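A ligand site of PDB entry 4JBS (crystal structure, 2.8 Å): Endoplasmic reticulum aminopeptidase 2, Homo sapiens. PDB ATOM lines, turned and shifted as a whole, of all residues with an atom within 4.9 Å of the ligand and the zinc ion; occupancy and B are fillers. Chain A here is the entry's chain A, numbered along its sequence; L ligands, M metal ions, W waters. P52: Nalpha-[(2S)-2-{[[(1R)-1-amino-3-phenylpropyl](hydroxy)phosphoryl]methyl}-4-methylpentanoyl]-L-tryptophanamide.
N2 of the ligand lies close to N of Gly 334 (3.2 Å).
The side-chain carboxylate of Glu 337 is in salt-bridge range of a nitrogen (N1) of the ligand.
N1 of the ligand is in salt-bridge range of OE1 of Glu 200, at 2.8 Å.
The side-chain hydroxyl (OH) of Tyr 455 lies close to an oxygen (O2) of the ligand, at 2.7 Å.
SD of Met 336 lies within hydrogen-bond range of N1 of the ligand (3.7 Å).
The side-chain amino group of Lys 392 lies close to a nitrogen (N1) of the ligand (3.4 Å).
OE1 of Glu 337 is in salt-bridge range of NZ of Lys 392, at 2.7 Å.
ND1 of His 370 sits at hydrogen-bond distance from OE2 of Glu 400.
The side-chain carboxylate (OE2) of Glu 393 lies within salt-bridge range of the side-chain amino group (NZ) of Lys 392.
The side-chain carboxylate of Glu 200 lies within salt-bridge range of the side-chain amino group of Lys 392.
The side-chain carboxylate (OE2) of Glu 393 sits close to the side-chain hydroxyl (OH) of Tyr 455, 3.1 Å away.
OE2 of Glu 371 is in hydrogen-bond range of N of Glu 337, 3.1 Å away.
An oxygen (O1) of the ligand lies close to the side-chain carboxylate (OE1) of Glu 371.
Ala 335 touches the ligand (O to C11, 2.9 Å).
CB of Val 367 touches C15 of the ligand, at 3.7 Å.
Phe 450 touches the ligand.
CA of Asp 451 touches C25 of the ligand, at 3.7 Å.
CZ of Tyr 892 touches C24 of the ligand, at 3.5 Å.
Residues that only touch the zinc ion: Tyr 455.
Four residues have an atom within 4 Å of the zinc ion: His 370, His 374, Glu 393 and Tyr 455.
The zinc ion is bound by the side-chain carboxylate of Glu 393 (2.0 Å), a ring nitrogen (NE2) of His 374 (2.1 Å), a ring nitrogen (NE2) of His 370 (2.1 Å), an oxygen (O2) of the ligand (2.2 Å) and an oxygen (O1) of the ligand (2.5 Å).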
ATOM      1  N   GLU A 200     -12.970  38.745  25.850  1.00  0.00           N
ATOM      2  CA  GLU A 200     -12.112  38.245  24.769  1.00  0.00           C
ATOM      3  C   GLU A 200     -12.839  38.187  23.432  1.00  0.00           C
ATOM      4  O   GLU A 200     -13.978  37.716  23.368  1.00  0.00           O
ATOM      5  CB  GLU A 200     -11.516  36.883  25.114  1.00  0.00           C
ATOM      6  CG  GLU A 200     -10.333  36.517  24.234  1.00  0.00           C
ATOM      7  CD  GLU A 200      -9.839  35.113  24.480  1.00  0.00           C
ATOM      8  OE1 GLU A 200     -10.526  34.373  25.209  1.00  0.00           O
ATOM      9  OE2 GLU A 200      -8.783  34.750  23.931  1.00  0.00           O
ATOM     10  N   PRO A 201     -12.186  38.659  22.355  1.00  0.00           N
ATOM     11  CA  PRO A 201     -10.860  39.269  22.439  1.00  0.00           C
ATOM     12  C   PRO A 201     -10.914  40.789  22.542  1.00  0.00           C
ATOM     13  O   PRO A 201     -10.024  41.408  23.130  1.00  0.00           O
ATOM     14  CB  PRO A 201     -10.221  38.884  21.086  1.00  0.00           C
ATOM     15  CG  PRO A 201     -11.298  38.177  20.287  1.00  0.00           C
ATOM     16  CD  PRO A 201     -12.601  38.466  20.964  1.00  0.00           C
ATOM     17  N   PRO A 333     -19.656  31.804  25.218  1.00  0.00           N
ATOM     18  CA  PRO A 333     -18.518  30.899  25.102  1.00  0.00           C
ATOM     19  C   PRO A 333     -18.750  29.631  25.913  1.00  0.00           C
ATOM     20  O   PRO A 333     -19.725  29.564  26.661  1.00  0.00           O
ATOM     21  CB  PRO A 333     -17.361  31.698  25.716  1.00  0.00           C
ATOM     22  CG  PRO A 333     -17.872  33.088  25.918  1.00  0.00           C
ATOM     23  CD  PRO A 333     -19.348  32.987  26.032  1.00  0.00           C
ATOM     24  N   GLY A 334     -17.879  28.628  25.763  1.00  0.00           N
ATOM     25  CA  GLY A 334     -17.950  27.448  26.597  1.00  0.00           C
ATOM     26  C   GLY A 334     -17.571  27.812  28.017  1.00  0.00           C
ATOM     27  O   GLY A 334     -18.197  27.362  28.980  1.00  0.00           O
ATOM     28  N   ALA A 335     -16.542  28.643  28.132  1.00  0.00           N
ATOM     29  CA  ALA A 335     -16.128  29.242  29.409  1.00  0.00           C
ATOM     30  C   ALA A 335     -15.062  30.318  29.136  1.00  0.00           C
ATOM     31  O   ALA A 335     -14.557  30.412  28.020  1.00  0.00           O
ATOM     32  CB  ALA A 335     -15.593  28.170  30.339  1.00  0.00           C
ATOM     33  N   MET A 336     -14.723  31.120  30.135  1.00  0.00           N
ATOM     34  CA  MET A 336     -13.678  32.141  29.974  1.00  0.00           C
ATOM     35  C   MET A 336     -12.719  32.201  31.157  1.00  0.00           C
ATOM     36  O   MET A 336     -13.128  32.206  32.321  1.00  0.00           O
ATOM     37  CB  MET A 336     -14.285  33.518  29.704  1.00  0.00           C
ATOM     38  CG  MET A 336     -13.245  34.615  29.486  1.00  0.00           C
ATOM     39  SD  MET A 336     -12.145  34.291  28.080  1.00  0.00           S
ATOM     40  CE  MET A 336     -10.833  35.483  28.376  1.00  0.00           C
ATOM     41  N   GLU A 337     -11.439  32.263  30.849  1.00  0.00           N
ATOM     42  CA  GLU A 337     -10.401  32.056  31.848  1.00  0.00           C
ATOM     43  C   GLU A 337     -10.011  33.308  32.626  1.00  0.00           C
ATOM     44  O   GLU A 337      -8.898  33.381  33.159  1.00  0.00           O
ATOM     45  CB  GLU A 337      -9.164  31.427  31.194  1.00  0.00           C
ATOM     46  CG  GLU A 337      -8.318  32.372  30.340  1.00  0.00           C
ATOM     47  CD  GLU A 337      -8.671  32.349  28.863  1.00  0.00           C
ATOM     48  OE1 GLU A 337      -7.832  32.809  28.043  1.00  0.00           O
ATOM     49  OE2 GLU A 337      -9.778  31.880  28.505  1.00  0.00           O
ATOM     50  N   TRP A 363     -16.690  15.727  30.358  1.00  0.00           N
ATOM     51  CA  TRP A 363     -16.772  17.071  29.797  1.00  0.00           C
ATOM     52  C   TRP A 363     -16.355  18.122  30.821  1.00  0.00           C
ATOM     53  O   TRP A 363     -15.328  18.794  30.630  1.00  0.00           O
ATOM     54  CB  TRP A 363     -18.194  17.371  29.302  1.00  0.00           C
ATOM     55  CG  TRP A 363     -18.401  18.783  28.743  1.00  0.00           C
ATOM     56  CD1 TRP A 363     -19.262  19.737  29.212  1.00  0.00           C
ATOM     57  CD2 TRP A 363     -17.740  19.361  27.605  1.00  0.00           C
ATOM     58  NE1 TRP A 363     -19.170  20.875  28.441  1.00  0.00           N
ATOM     59  CE2 TRP A 363     -18.242  20.672  27.459  1.00  0.00           C
ATOM     60  CE3 TRP A 363     -16.768  18.904  26.718  1.00  0.00           C
ATOM     61  CZ2 TRP A 363     -17.801  21.520  26.435  1.00  0.00           C
ATOM     62  CZ3 TRP A 363     -16.334  19.756  25.706  1.00  0.00           C
ATOM     63  CH2 TRP A 363     -16.856  21.050  25.570  1.00  0.00           C
ATOM     64  N   VAL A 367     -13.203  20.720  30.589  1.00  0.00           N
ATOM     65  CA  VAL A 367     -13.262  22.179  30.485  1.00  0.00           C
ATOM     66  C   VAL A 367     -12.701  22.894  31.713  1.00  0.00           C
ATOM     67  O   VAL A 367     -12.122  23.972  31.611  1.00  0.00           O
ATOM     68  CB  VAL A 367     -14.675  22.713  30.084  1.00  0.00           C
ATOM     69  CG1 VAL A 367     -15.746  21.701  30.391  1.00  0.00           C
ATOM     70  CG2 VAL A 367     -14.967  24.052  30.742  1.00  0.00           C
ATOM     71  N   HIS A 370      -9.023  22.702  31.213  1.00  0.00           N
ATOM     72  CA  HIS A 370      -8.695  23.697  30.205  1.00  0.00           C
ATOM     73  C   HIS A 370      -8.532  25.091  30.792  1.00  0.00           C
ATOM     74  O   HIS A 370      -7.538  25.776  30.541  1.00  0.00           O
ATOM     75  CB  HIS A 370      -9.767  23.724  29.112  1.00  0.00           C
ATOM     76  CG  HIS A 370      -9.410  24.559  27.920  1.00  0.00           C
ATOM     77  ND1 HIS A 370      -8.641  24.080  26.891  1.00  0.00           N
ATOM     78  CD2 HIS A 370      -9.745  25.831  27.586  1.00  0.00           C
ATOM     79  CE1 HIS A 370      -8.506  25.025  25.965  1.00  0.00           C
ATOM     80  NE2 HIS A 370      -9.174  26.087  26.365  1.00  0.00           N
ATOM     81  N   GLU A 371      -9.508  25.528  31.589  1.00  0.00           N
ATOM     82  CA  GLU A 371      -9.511  26.902  32.099  1.00  0.00           C
ATOM     83  C   GLU A 371      -8.412  27.147  33.125  1.00  0.00           C
ATOM     84  O   GLU A 371      -7.839  28.232  33.164  1.00  0.00           O
ATOM     85  CB  GLU A 371     -10.869  27.275  32.676  1.00  0.00           C
ATOM     86  CG  GLU A 371     -12.017  27.132  31.695  1.00  0.00           C
ATOM     87  CD  GLU A 371     -11.860  28.005  30.471  1.00  0.00           C
ATOM     88  OE1 GLU A 371     -12.227  27.538  29.366  1.00  0.00           O
ATOM     89  OE2 GLU A 371     -11.374  29.143  30.593  1.00  0.00           O
ATOM     90  N   HIS A 374      -5.118  27.771  31.672  1.00  0.00           N
ATOM     91  CA  HIS A 374      -5.059  29.114  31.092  1.00  0.00           C
ATOM     92  C   HIS A 374      -4.429  30.120  32.038  1.00  0.00           C
ATOM     93  O   HIS A 374      -3.724  31.033  31.595  1.00  0.00           O
ATOM     94  CB  HIS A 374      -6.462  29.602  30.714  1.00  0.00           C
ATOM     95  CG  HIS A 374      -6.824  29.319  29.284  1.00  0.00           C
ATOM     96  ND1 HIS A 374      -5.901  29.326  28.265  1.00  0.00           N
ATOM     97  CD2 HIS A 374      -8.022  29.035  28.715  1.00  0.00           C
ATOM     98  CE1 HIS A 374      -6.514  29.046  27.124  1.00  0.00           C
ATOM     99  NE2 HIS A 374      -7.799  28.878  27.371  1.00  0.00           N
ATOM    100  N   LYS A 392      -1.739  30.088  23.513  1.00  0.00           N
ATOM    101  CA  LYS A 392      -2.645  30.059  24.654  1.00  0.00           C
ATOM    102  C   LYS A 392      -3.556  28.848  24.524  1.00  0.00           C
ATOM    103  O   LYS A 392      -3.631  28.011  25.429  1.00  0.00           O
ATOM    104  CB  LYS A 392      -3.459  31.355  24.678  1.00  0.00           C
ATOM    105  CG  LYS A 392      -4.431  31.516  25.840  1.00  0.00           C
ATOM    106  CD  LYS A 392      -4.963  32.954  25.932  1.00  0.00           C
ATOM    107  CE  LYS A 392      -6.069  33.232  24.918  1.00  0.00           C
ATOM    108  NZ  LYS A 392      -7.399  32.753  25.392  1.00  0.00           N
ATOM    109  N   GLU A 393      -4.220  28.740  23.383  1.00  0.00           N
ATOM    110  CA  GLU A 393      -5.256  27.731  23.155  1.00  0.00           C
ATOM    111  C   GLU A 393      -4.772  26.312  22.895  1.00  0.00           C
ATOM    112  O   GLU A 393      -5.332  25.356  23.443  1.00  0.00           O
ATOM    113  CB  GLU A 393      -6.181  28.197  22.025  1.00  0.00           C
ATOM    114  CG  GLU A 393      -6.914  29.487  22.345  1.00  0.00           C
ATOM    115  CD  GLU A 393      -7.729  29.391  23.636  1.00  0.00           C
ATOM    116  OE1 GLU A 393      -7.882  28.270  24.146  1.00  0.00           O
ATOM    117  OE2 GLU A 393      -8.212  30.433  24.122  1.00  0.00           O
ATOM    118  N   ALA A 396      -3.418  24.983  26.369  1.00  0.00           N
ATOM    119  CA  ALA A 396      -4.508  24.668  27.277  1.00  0.00           C
ATOM    120  C   ALA A 396      -5.182  23.366  26.848  1.00  0.00           C
ATOM    121  O   ALA A 396      -5.381  22.467  27.656  1.00  0.00           O
ATOM    122  CB  ALA A 396      -5.521  25.798  27.293  1.00  0.00           C
ATOM    123  N   GLU A 400      -5.149  19.710  29.012  1.00  0.00           N
ATOM    124  CA  GLU A 400      -6.361  18.944  29.342  1.00  0.00           C
ATOM    125  C   GLU A 400      -5.961  17.485  29.480  1.00  0.00           C
ATOM    126  O   GLU A 400      -6.262  16.834  30.474  1.00  0.00           O
ATOM    127  CB  GLU A 400      -7.408  19.058  28.224  1.00  0.00           C
ATOM    128  CG  GLU A 400      -8.144  20.393  28.125  1.00  0.00           C
ATOM    129  CD  GLU A 400      -9.220  20.370  27.039  1.00  0.00           C
ATOM    130  OE1 GLU A 400      -9.678  19.265  26.679  1.00  0.00           O
ATOM    131  OE2 GLU A 400      -9.610  21.448  26.535  1.00  0.00           O
ATOM    132  N   PHE A 450     -10.083  31.425  16.362  1.00  0.00           N
ATOM    133  CA  PHE A 450     -10.445  30.427  17.358  1.00  0.00           C
ATOM    134  C   PHE A 450     -11.111  29.253  16.687  1.00  0.00           C
ATOM    135  O   PHE A 450     -12.299  29.276  16.394  1.00  0.00           O
ATOM    136  CB  PHE A 450     -11.379  31.037  18.413  1.00  0.00           C
ATOM    137  CG  PHE A 450     -10.740  32.125  19.230  1.00  0.00           C
ATOM    138  CD1 PHE A 450      -9.953  31.808  20.316  1.00  0.00           C
ATOM    139  CD2 PHE A 450     -10.923  33.447  18.902  1.00  0.00           C
ATOM    140  CE1 PHE A 450      -9.370  32.803  21.072  1.00  0.00           C
ATOM    141  CE2 PHE A 450     -10.330  34.450  19.652  1.00  0.00           C
ATOM    142  CZ  PHE A 450      -9.556  34.121  20.734  1.00  0.00           C
ATOM    143  N   ASP A 451     -10.335  28.214  16.424  1.00  0.00           N
ATOM    144  CA  ASP A 451     -10.862  27.055  15.719  1.00  0.00           C
ATOM    145  C   ASP A 451     -10.012  25.825  15.979  1.00  0.00           C
ATOM    146  O   ASP A 451      -9.078  25.857  16.774  1.00  0.00           O
ATOM    147  CB  ASP A 451     -10.944  27.344  14.224  1.00  0.00           C
ATOM    148  CG  ASP A 451      -9.582  27.478  13.583  1.00  0.00           C
ATOM    149  OD1 ASP A 451      -8.571  27.315  14.280  1.00  0.00           O
ATOM    150  OD2 ASP A 451      -9.547  27.753  12.366  1.00  0.00           O
ATOM    151  N   GLU A 452     -10.339  24.739  15.291  1.00  0.00           N
ATOM    152  CA  GLU A 452      -9.695  23.459  15.540  1.00  0.00           C
ATOM    153  C   GLU A 452      -8.251  23.416  15.068  1.00  0.00           C
ATOM    154  O   GLU A 452      -7.570  22.407  15.248  1.00  0.00           O
ATOM    155  CB  GLU A 452     -10.514  22.335  14.939  1.00  0.00           C
ATOM    156  CG  GLU A 452     -11.577  22.827  13.993  1.00  0.00           C
ATOM    157  CD  GLU A 452     -12.911  22.194  14.269  1.00  0.00           C
ATOM    158  OE1 GLU A 452     -12.990  20.947  14.297  1.00  0.00           O
ATOM    159  OE2 GLU A 452     -13.890  22.946  14.479  1.00  0.00           O
ATOM    160  N   TYR A 455      -6.553  25.267  18.278  1.00  0.00           N
ATOM    161  CA  TYR A 455      -6.850  24.425  19.422  1.00  0.00           C
ATOM    162  C   TYR A 455      -6.349  22.989  19.240  1.00  0.00           C
ATOM    163  O   TYR A 455      -5.367  22.585  19.851  1.00  0.00           O
ATOM    164  CB  TYR A 455      -8.352  24.420  19.720  1.00  0.00           C
ATOM    165  CG  TYR A 455      -8.885  25.663  20.414  1.00  0.00           C
ATOM    166  CD1 TYR A 455      -8.884  26.894  19.780  1.00  0.00           C
ATOM    167  CD2 TYR A 455      -9.386  25.589  21.707  1.00  0.00           C
ATOM    168  CE1 TYR A 455      -9.370  28.023  20.422  1.00  0.00           C
ATOM    169  CE2 TYR A 455      -9.885  26.716  22.343  1.00  0.00           C
ATOM    170  CZ  TYR A 455      -9.877  27.924  21.704  1.00  0.00           C
ATOM    171  OH  TYR A 455     -10.366  29.040  22.340  1.00  0.00           O
ATOM    172  N   TYR A 892     -18.625  32.213  17.070  1.00  0.00           N
ATOM    173  CA  TYR A 892     -18.741  30.774  16.911  1.00  0.00           C
ATOM    174  C   TYR A 892     -20.174  30.398  16.571  1.00  0.00           C
ATOM    175  O   TYR A 892     -20.412  29.478  15.790  1.00  0.00           O
ATOM    176  CB  TYR A 892     -18.296  30.029  18.162  1.00  0.00           C
ATOM    177  CG  TYR A 892     -18.023  28.566  17.911  1.00  0.00           C
ATOM    178  CD1 TYR A 892     -16.855  28.153  17.292  1.00  0.00           C
ATOM    179  CD2 TYR A 892     -18.943  27.590  18.306  1.00  0.00           C
ATOM    180  CE1 TYR A 892     -16.604  26.815  17.061  1.00  0.00           C
ATOM    181  CE2 TYR A 892     -18.692  26.252  18.074  1.00  0.00           C
ATOM    182  CZ  TYR A 892     -17.524  25.867  17.445  1.00  0.00           C
ATOM    183  OH  TYR A 892     -17.280  24.533  17.225  1.00  0.00           O
ATOM    184  N   ARG A 895     -20.687  31.166  12.785  1.00  0.00           N
ATOM    185  CA  ARG A 895     -19.838  30.270  12.026  1.00  0.00           C
ATOM    186  C   ARG A 895     -20.399  28.855  12.073  1.00  0.00           C
ATOM    187  O   ARG A 895     -20.331  28.103  11.105  1.00  0.00           O
ATOM    188  CB  ARG A 895     -18.410  30.273  12.570  1.00  0.00           C
ATOM    189  CG  ARG A 895     -17.625  29.033  12.186  1.00  0.00           C
ATOM    190  CD  ARG A 895     -16.129  29.259  12.220  1.00  0.00           C
ATOM    191  NE  ARG A 895     -15.549  28.939  13.519  1.00  0.00           N
ATOM    192  CZ  ARG A 895     -14.958  29.822  14.321  1.00  0.00           C
ATOM    193  NH1 ARG A 895     -14.869  31.096  13.942  1.00  0.00           N
ATOM    194  NH2 ARG A 895     -14.471  29.445  15.479  1.00  0.00           N
HETATM  195  O1  P52 L   1     -10.800  29.074  27.338  1.00  0.00           O
HETATM  196  O2  P52 L   1     -10.887  28.641  24.984  1.00  0.00           O
HETATM  197  C1  P52 L   1     -13.427  32.166  24.670  1.00  0.00           C
HETATM  198  C2  P52 L   1     -13.659  32.776  23.295  1.00  0.00           C
HETATM  199  C3  P52 L   1     -13.365  34.082  22.934  1.00  0.00           C
HETATM  200  C4  P52 L   1     -13.626  34.484  21.627  1.00  0.00           C
HETATM  201  C5  P52 L   1     -14.152  33.673  20.673  1.00  0.00           C
HETATM  202  C6  P52 L   1     -14.453  32.342  21.021  1.00  0.00           C
HETATM  203  N1  P52 L   1     -10.619  31.662  25.932  1.00  0.00           N
HETATM  204  C7  P52 L   1     -14.201  31.922  22.338  1.00  0.00           C
HETATM  205  C8  P52 L   1     -12.264  31.188  24.560  1.00  0.00           C
HETATM  206  C9  P52 L   1     -11.725  31.014  25.788  1.00  0.00           C
HETATM  207  C10 P52 L   1     -13.997  28.052  23.991  1.00  0.00           C
HETATM  208  C11 P52 L   1     -13.025  28.667  26.316  1.00  0.00           C
HETATM  209  C12 P52 L   1     -13.332  27.549  25.261  1.00  0.00           C
HETATM  210  N2  P52 L   1     -15.400  27.885  23.801  1.00  0.00           N
HETATM  211  C13 P52 L   1     -14.238  26.469  25.937  1.00  0.00           C
HETATM  212  C14 P52 L   1     -13.752  25.023  25.785  1.00  0.00           C
HETATM  213  C15 P52 L   1     -13.318  24.427  27.130  1.00  0.00           C
HETATM  214  C16 P52 L   1     -12.587  25.028  24.785  1.00  0.00           C
HETATM  215  C17 P52 L   1     -16.468  27.210  23.064  1.00  0.00           C
HETATM  216  N3  P52 L   1     -13.368  28.437  19.976  1.00  0.00           N
HETATM  217  P1  P52 L   1     -11.563  29.277  26.109  1.00  0.00           P
HETATM  218  C18 P52 L   1     -16.227  25.703  22.958  1.00  0.00           C
HETATM  219  C19 P52 L   1     -16.604  27.809  21.666  1.00  0.00           C
HETATM  220  C20 P52 L   1     -15.324  27.794  20.891  1.00  0.00           C
HETATM  221  C21 P52 L   1     -14.441  28.824  20.741  1.00  0.00           C
HETATM  222  C22 P52 L   1     -14.762  26.686  20.165  1.00  0.00           C
HETATM  223  C23 P52 L   1     -13.542  27.118  19.607  1.00  0.00           C
HETATM  224  C24 P52 L   1     -15.173  25.368  19.929  1.00  0.00           C
HETATM  225  C25 P52 L   1     -12.730  26.294  18.835  1.00  0.00           C
HETATM  226  C26 P52 L   1     -14.361  24.534  19.160  1.00  0.00           C
HETATM  227  C27 P52 L   1     -13.151  25.006  18.624  1.00  0.00           C
HETATM  228  O4  P52 L   1     -15.081  25.264  22.901  1.00  0.00           O
HETATM  229  N4  P52 L   1     -17.319  24.811  22.782  1.00  0.00           N
HETATM  230 ZN    ZN M   1      -8.974  28.100  25.869  1.00  0.00          ZN
HETATM  231  O   HOH W   1     -15.947  22.627  21.993  1.00  0.00           O
HETATM  232  O   HOH W   2     -15.021  35.891  25.330  1.00  0.00           O
HETATM  233  O   HOH W   3     -19.391  25.852  23.720  1.00  0.00           O
